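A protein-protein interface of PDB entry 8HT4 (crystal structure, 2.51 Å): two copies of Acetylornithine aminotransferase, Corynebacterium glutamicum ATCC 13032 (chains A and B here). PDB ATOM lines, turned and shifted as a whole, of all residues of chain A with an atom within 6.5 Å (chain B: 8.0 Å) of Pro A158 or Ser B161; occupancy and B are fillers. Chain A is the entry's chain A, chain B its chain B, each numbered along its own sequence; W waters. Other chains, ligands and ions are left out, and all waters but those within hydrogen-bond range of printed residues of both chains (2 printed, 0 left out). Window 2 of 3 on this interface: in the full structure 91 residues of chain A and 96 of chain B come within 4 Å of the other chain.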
ATOM      1  N   MET A 141      22.699   2.337  -6.081  1.00  0.00           N
ATOM      2  CA  MET A 141      22.884   3.434  -5.098  1.00  0.00           C
ATOM      3  C   MET A 141      24.316   3.440  -4.529  1.00  0.00           C
ATOM      4  O   MET A 141      24.898   4.549  -4.354  1.00  0.00           O
ATOM      5  CB  MET A 141      21.817   3.336  -4.006  1.00  0.00           C
ATOM      6  CG  MET A 141      20.496   4.001  -4.428  1.00  0.00           C
ATOM      7  SD  MET A 141      20.607   5.827  -4.439  1.00  0.00           S
ATOM      8  CE  MET A 141      19.092   6.239  -5.283  1.00  0.00           C
ATOM      9  N   GLU A 154      22.649  13.904  -7.937  1.00  0.00           N
ATOM     10  CA  GLU A 154      21.833  14.964  -7.272  1.00  0.00           C
ATOM     11  C   GLU A 154      20.424  14.442  -7.027  1.00  0.00           C
ATOM     12  O   GLU A 154      20.026  14.331  -5.864  1.00  0.00           O
ATOM     13  CB  GLU A 154      21.666  16.225  -8.123  1.00  0.00           C
ATOM     14  CG  GLU A 154      22.776  17.245  -7.949  1.00  0.00           C
ATOM     15  CD  GLU A 154      23.320  17.419  -6.537  1.00  0.00           C
ATOM     16  OE1 GLU A 154      22.599  18.035  -5.679  1.00  0.00           O
ATOM     17  OE2 GLU A 154      24.466  16.922  -6.291  1.00  0.00           O
ATOM     18  N   PHE A 156      19.073  11.819  -6.666  1.00  0.00           N
ATOM     19  CA  PHE A 156      18.857  10.621  -5.810  1.00  0.00           C
ATOM     20  C   PHE A 156      19.452  10.727  -4.413  1.00  0.00           C
ATOM     21  O   PHE A 156      19.541   9.714  -3.737  1.00  0.00           O
ATOM     22  CB  PHE A 156      19.387   9.414  -6.576  1.00  0.00           C
ATOM     23  CG  PHE A 156      18.954   9.394  -8.014  1.00  0.00           C
ATOM     24  CD1 PHE A 156      17.673   9.002  -8.346  1.00  0.00           C
ATOM     25  CD2 PHE A 156      19.804   9.819  -9.020  1.00  0.00           C
ATOM     26  CE1 PHE A 156      17.263   8.997  -9.663  1.00  0.00           C
ATOM     27  CE2 PHE A 156      19.382   9.830 -10.335  1.00  0.00           C
ATOM     28  CZ  PHE A 156      18.110   9.427 -10.649  1.00  0.00           C
ATOM     29  N   LEU A 157      19.776  11.933  -3.985  1.00  0.00           N
ATOM     30  CA  LEU A 157      20.309  12.175  -2.625  1.00  0.00           C
ATOM     31  C   LEU A 157      19.213  11.914  -1.579  1.00  0.00           C
ATOM     32  O   LEU A 157      18.053  12.154  -1.867  1.00  0.00           O
ATOM     33  CB  LEU A 157      20.786  13.629  -2.590  1.00  0.00           C
ATOM     34  CG  LEU A 157      22.278  13.925  -2.732  1.00  0.00           C
ATOM     35  CD1 LEU A 157      22.997  12.894  -3.572  1.00  0.00           C
ATOM     36  CD2 LEU A 157      22.477  15.306  -3.324  1.00  0.00           C
ATOM     37  N   PRO A 158      19.538  11.480  -0.353  1.00  0.00           N
ATOM     38  CA  PRO A 158      20.913  11.213   0.060  1.00  0.00           C
ATOM     39  C   PRO A 158      21.579   9.920  -0.434  1.00  0.00           C
ATOM     40  O   PRO A 158      20.941   8.907  -0.547  1.00  0.00           O
ATOM     41  CB  PRO A 158      20.845  11.229   1.591  1.00  0.00           C
ATOM     42  CG  PRO A 158      19.459  11.703   1.929  1.00  0.00           C
ATOM     43  CD  PRO A 158      18.615  11.287   0.751  1.00  0.00           C
ATOM     44  N   MET A 159      22.874  10.001  -0.695  1.00  0.00           N
ATOM     45  CA  MET A 159      23.649   8.812  -1.109  1.00  0.00           C
ATOM     46  C   MET A 159      24.088   8.008   0.103  1.00  0.00           C
ATOM     47  O   MET A 159      24.194   8.598   1.181  1.00  0.00           O
ATOM     48  CB  MET A 159      24.939   9.248  -1.807  1.00  0.00           C
ATOM     49  CG  MET A 159      24.772   9.851  -3.176  1.00  0.00           C
ATOM     50  SD  MET A 159      24.444   8.664  -4.482  1.00  0.00           S
ATOM     51  CE  MET A 159      22.700   8.982  -4.707  1.00  0.00           C
ATOM     52  N   PRO A 160      24.306   6.679  -0.028  1.00  0.00           N
ATOM     53  CA  PRO A 160      24.943   5.910   1.030  1.00  0.00           C
ATOM     54  C   PRO A 160      26.218   6.699   1.385  1.00  0.00           C
ATOM     55  O   PRO A 160      26.984   6.958   0.495  1.00  0.00           O
ATOM     56  CB  PRO A 160      25.207   4.528   0.423  1.00  0.00           C
ATOM     57  CG  PRO A 160      24.766   4.610  -1.015  1.00  0.00           C
ATOM     58  CD  PRO A 160      23.916   5.851  -1.162  1.00  0.00           C
ATOM     59  N   SER A 161      26.437   7.007   2.668  1.00  0.00           N
ATOM     60  CA  SER A 161      27.541   7.902   3.118  1.00  0.00           C
ATOM     61  C   SER A 161      28.953   7.338   3.025  1.00  0.00           C
ATOM     62  O   SER A 161      29.097   6.124   2.965  1.00  0.00           O
ATOM     63  CB  SER A 161      27.291   8.368   4.522  1.00  0.00           C
ATOM     64  OG  SER A 161      28.038   7.609   5.453  1.00  0.00           O
ATOM     65  N   PHE B 118      13.748   2.123  -6.059  1.00  0.00           N
ATOM     66  CA  PHE B 118      14.286   3.001  -4.984  1.00  0.00           C
ATOM     67  C   PHE B 118      14.527   4.406  -5.564  1.00  0.00           C
ATOM     68  O   PHE B 118      14.200   5.420  -4.903  1.00  0.00           O
ATOM     69  CB  PHE B 118      15.559   2.387  -4.386  1.00  0.00           C
ATOM     70  CG  PHE B 118      16.171   3.134  -3.226  1.00  0.00           C
ATOM     71  CD1 PHE B 118      16.898   4.295  -3.430  1.00  0.00           C
ATOM     72  CD2 PHE B 118      16.042   2.657  -1.932  1.00  0.00           C
ATOM     73  CE1 PHE B 118      17.466   4.981  -2.363  1.00  0.00           C
ATOM     74  CE2 PHE B 118      16.575   3.361  -0.856  1.00  0.00           C
ATOM     75  CZ  PHE B 118      17.308   4.516  -1.073  1.00  0.00           C
ATOM     76  N   ARG B 122      13.143   8.189  -4.831  1.00  0.00           N
ATOM     77  CA  ARG B 122      13.954   9.377  -4.479  1.00  0.00           C
ATOM     78  C   ARG B 122      13.559  10.544  -5.381  1.00  0.00           C
ATOM     79  O   ARG B 122      13.669  11.685  -4.936  1.00  0.00           O
ATOM     80  CB  ARG B 122      15.433   9.045  -4.677  1.00  0.00           C
ATOM     81  CG  ARG B 122      16.074   8.282  -3.533  1.00  0.00           C
ATOM     82  CD  ARG B 122      16.402   9.243  -2.418  1.00  0.00           C
ATOM     83  NE  ARG B 122      17.488   8.773  -1.583  1.00  0.00           N
ATOM     84  CZ  ARG B 122      17.322   8.114  -0.450  1.00  0.00           C
ATOM     85  NH1 ARG B 122      18.375   7.725   0.243  1.00  0.00           N
ATOM     86  NH2 ARG B 122      16.107   7.832  -0.022  1.00  0.00           N
ATOM     87  N   ARG B 126      10.279  13.314  -1.947  1.00  0.00           N
ATOM     88  CA  ARG B 126       9.942  12.824  -0.578  1.00  0.00           C
ATOM     89  C   ARG B 126      11.056  11.911  -0.038  1.00  0.00           C
ATOM     90  O   ARG B 126      11.704  11.191  -0.845  1.00  0.00           O
ATOM     91  CB  ARG B 126       8.620  12.052  -0.584  1.00  0.00           C
ATOM     92  CG  ARG B 126       7.473  12.806  -1.239  1.00  0.00           C
ATOM     93  CD  ARG B 126       6.142  12.141  -0.971  1.00  0.00           C
ATOM     94  NE  ARG B 126       5.039  12.992  -1.403  1.00  0.00           N
ATOM     95  CZ  ARG B 126       3.747  12.698  -1.280  1.00  0.00           C
ATOM     96  NH1 ARG B 126       3.355  11.554  -0.742  1.00  0.00           N
ATOM     97  NH2 ARG B 126       2.844  13.559  -1.697  1.00  0.00           N
ATOM     98  N   SER B 127      11.249  11.910   1.288  1.00  0.00           N
ATOM     99  CA  SER B 127      12.422  11.316   1.974  1.00  0.00           C
ATOM    100  C   SER B 127      12.118   9.905   2.518  1.00  0.00           C
ATOM    101  O   SER B 127      13.031   9.049   2.517  1.00  0.00           O
ATOM    102  CB  SER B 127      12.917  12.270   3.045  1.00  0.00           C
ATOM    103  OG  SER B 127      12.236  12.063   4.275  1.00  0.00           O
ATOM    104  N   ARG B 128      10.892   9.639   2.953  1.00  0.00           N
ATOM    105  CA  ARG B 128      10.535   8.385   3.667  1.00  0.00           C
ATOM    106  C   ARG B 128      10.140   7.309   2.654  1.00  0.00           C
ATOM    107  O   ARG B 128       9.363   7.605   1.738  1.00  0.00           O
ATOM    108  CB  ARG B 128       9.385   8.608   4.647  1.00  0.00           C
ATOM    109  CG  ARG B 128       9.636   9.693   5.686  1.00  0.00           C
ATOM    110  CD  ARG B 128       8.405   9.891   6.548  1.00  0.00           C
ATOM    111  NE  ARG B 128       8.190   8.752   7.428  1.00  0.00           N
ATOM    112  CZ  ARG B 128       7.019   8.332   7.916  1.00  0.00           C
ATOM    113  NH1 ARG B 128       5.885   8.951   7.626  1.00  0.00           N
ATOM    114  NH2 ARG B 128       7.000   7.292   8.731  1.00  0.00           N
ATOM    115  N   ILE B 129      10.690   6.108   2.811  1.00  0.00           N
ATOM    116  CA  ILE B 129      10.309   4.875   2.068  1.00  0.00           C
ATOM    117  C   ILE B 129       9.996   3.846   3.140  1.00  0.00           C
ATOM    118  O   ILE B 129      10.848   3.691   4.039  1.00  0.00           O
ATOM    119  CB  ILE B 129      11.436   4.382   1.138  1.00  0.00           C
ATOM    120  CG1 ILE B 129      11.746   5.383   0.026  1.00  0.00           C
ATOM    121  CG2 ILE B 129      11.121   3.010   0.574  1.00  0.00           C
ATOM    122  CD1 ILE B 129      13.112   5.190  -0.531  1.00  0.00           C
ATOM    123  N   MET B 141      23.202  -1.808  -2.120  1.00  0.00           N
ATOM    124  CA  MET B 141      23.081  -0.849  -0.984  1.00  0.00           C
ATOM    125  C   MET B 141      21.660  -0.248  -0.922  1.00  0.00           C
ATOM    126  O   MET B 141      21.157  -0.048   0.183  1.00  0.00           O
ATOM    127  CB  MET B 141      24.135   0.262  -1.105  1.00  0.00           C
ATOM    128  CG  MET B 141      25.555  -0.182  -0.737  1.00  0.00           C
ATOM    129  SD  MET B 141      25.859  -0.441   1.045  1.00  0.00           S
ATOM    130  CE  MET B 141      25.390  -2.159   1.188  1.00  0.00           C
ATOM    131  N   ALA B 145      19.023  -1.597   1.749  1.00  0.00           N
ATOM    132  CA  ALA B 145      18.334  -0.523   2.495  1.00  0.00           C
ATOM    133  C   ALA B 145      16.877  -0.924   2.731  1.00  0.00           C
ATOM    134  O   ALA B 145      16.421  -0.811   3.883  1.00  0.00           O
ATOM    135  CB  ALA B 145      18.425   0.755   1.716  1.00  0.00           C
ATOM    136  N   PRO B 158      26.917   2.959   7.171  1.00  0.00           N
ATOM    137  CA  PRO B 158      25.576   3.479   6.880  1.00  0.00           C
ATOM    138  C   PRO B 158      24.836   3.125   5.580  1.00  0.00           C
ATOM    139  O   PRO B 158      25.417   3.144   4.539  1.00  0.00           O
ATOM    140  CB  PRO B 158      25.738   4.999   7.045  1.00  0.00           C
ATOM    141  CG  PRO B 158      27.102   5.183   7.639  1.00  0.00           C
ATOM    142  CD  PRO B 158      27.896   4.027   7.085  1.00  0.00           C
ATOM    143  N   MET B 159      23.551   2.812   5.707  1.00  0.00           N
ATOM    144  CA  MET B 159      22.677   2.523   4.548  1.00  0.00           C
ATOM    145  C   MET B 159      22.219   3.811   3.871  1.00  0.00           C
ATOM    146  O   MET B 159      22.318   4.863   4.491  1.00  0.00           O
ATOM    147  CB  MET B 159      21.394   1.854   5.055  1.00  0.00           C
ATOM    148  CG  MET B 159      21.541   0.444   5.545  1.00  0.00           C
ATOM    149  SD  MET B 159      21.581  -0.761   4.226  1.00  0.00           S
ATOM    150  CE  MET B 159      23.252  -1.359   4.442  1.00  0.00           C
ATOM    151  N   PRO B 160      21.768   3.775   2.603  1.00  0.00           N
ATOM    152  CA  PRO B 160      21.121   4.940   2.012  1.00  0.00           C
ATOM    153  C   PRO B 160      19.954   5.249   2.968  1.00  0.00           C
ATOM    154  O   PRO B 160      19.181   4.354   3.202  1.00  0.00           O
ATOM    155  CB  PRO B 160      20.743   4.489   0.599  1.00  0.00           C
ATOM    156  CG  PRO B 160      21.548   3.248   0.327  1.00  0.00           C
ATOM    157  CD  PRO B 160      21.940   2.674   1.668  1.00  0.00           C
ATOM    158  N   SER B 161      19.815   6.504   3.366  1.00  0.00           N
ATOM    159  CA  SER B 161      18.817   6.896   4.380  1.00  0.00           C
ATOM    160  C   SER B 161      17.386   6.970   3.879  1.00  0.00           C
ATOM    161  O   SER B 161      17.188   7.212   2.703  1.00  0.00           O
ATOM    162  CB  SER B 161      19.204   8.212   4.955  1.00  0.00           C
ATOM    163  OG  SER B 161      18.744   9.271   4.142  1.00  0.00           O
ATOM    164  N   GLY B 162      16.439   6.649   4.755  1.00  0.00           N
ATOM    165  CA  GLY B 162      15.029   6.932   4.445  1.00  0.00           C
ATOM    166  C   GLY B 162      14.134   5.738   4.664  1.00  0.00           C
ATOM    167  O   GLY B 162      12.903   5.922   4.587  1.00  0.00           O
ATOM    168  N   VAL B 163      14.697   4.567   4.958  1.00  0.00           N
ATOM    169  CA  VAL B 163      13.872   3.330   5.053  1.00  0.00           C
ATOM    170  C   VAL B 163      13.405   3.156   6.498  1.00  0.00           C
ATOM    171  O   VAL B 163      14.182   3.384   7.456  1.00  0.00           O
ATOM    172  CB  VAL B 163      14.571   2.079   4.485  1.00  0.00           C
ATOM    173  CG1 VAL B 163      13.645   0.870   4.493  1.00  0.00           C
ATOM    174  CG2 VAL B 163      15.073   2.337   3.069  1.00  0.00           C
ATOM    175  N   GLU B 164      12.121   2.849   6.620  1.00  0.00           N
ATOM    176  CA  GLU B 164      11.441   2.514   7.886  1.00  0.00           C
ATOM    177  C   GLU B 164      10.638   1.252   7.622  1.00  0.00           C
ATOM    178  O   GLU B 164      10.099   1.133   6.509  1.00  0.00           O
ATOM    179  CB  GLU B 164      10.530   3.647   8.365  1.00  0.00           C
ATOM    180  CG  GLU B 164      11.219   4.982   8.504  1.00  0.00           C
ATOM    181  CD  GLU B 164      10.225   6.110   8.690  1.00  0.00           C
ATOM    182  OE1 GLU B 164       9.448   6.015   9.644  1.00  0.00           O
ATOM    183  OE2 GLU B 164      10.224   7.072   7.871  1.00  0.00           O
HETATM  184  O   HOH W   1      22.039   8.280   2.942  1.00  0.00           O
HETATM  185  O   HOH W   2      24.215   6.737   4.322  1.00  0.00           O
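NH1 of Arg B122 is in hydrogen-bond range of O of Pro A158, 2.9 Å away.
The guanidinium group of Arg B122 lies close to the backbone carbonyl oxygen of Leu A157 (3.4 Å).
O of Phe A156 lies within hydrogen-bond range of NE of Arg B122, at 3.1 Å.
The guanidinium group of Arg B122 lies within hydrogen-bond range of the backbone carbonyl oxygen of Ser B161 (2.8 Å).
Among the printed residues, pairs that only touch across the chains: Met A141 with Phe B118 (3.5 Å), Pro A158 with Ser B161 (3.4 Å), Pro A160 with Pro B160 (3.7 Å) and Ser A161 with Pro B158 (3.4 Å).
Printed residues of chain B within 4 Å of Met A141: Phe B118.
Of the printed residues of chain B, Leu A157 touches Arg B122.
Of chain B, only Arg B122 and Ser B161 come within 4 Å of Pro A158.
Printed residues of chain A within 4 Å of Pro B160: Pro A160.
Ser B161 touches just one residue of chain A: Pro A158 (3.4 Å).
The nearest residue of chain B that does not touch Pro A158 is Pro B160 (4.6 Å).
Of the 15 printed residues of chain B, 5 touch a printed residue of chain A.
Hydrophobic or aromatic side chains of chain A that line the printed part of chain B: Met A141, Pro A158 and Pro A160.
Pro A158 touches Ser B161, and with the chains exchanged Ser A161 touches Pro B158.
Pro B160 touches its own counterpart, Pro A160.
Positions printed for both chains: 141, 158, 159, 160 and 161.
Of the 7 pairs that touch across the chains among the printed residues, 3 have their exchanged pair printed and touching as well.
Water W2 bridges the backbone carbonyl oxygen (O) of Met B159 (2.7 Å) and the backbone NH (N) of Ser A161 (2.8 Å).
Water W1 lies within hydrogen-bond range of O of Met A159 (2.8 Å) and N of Ser B161 (2.9 Å).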
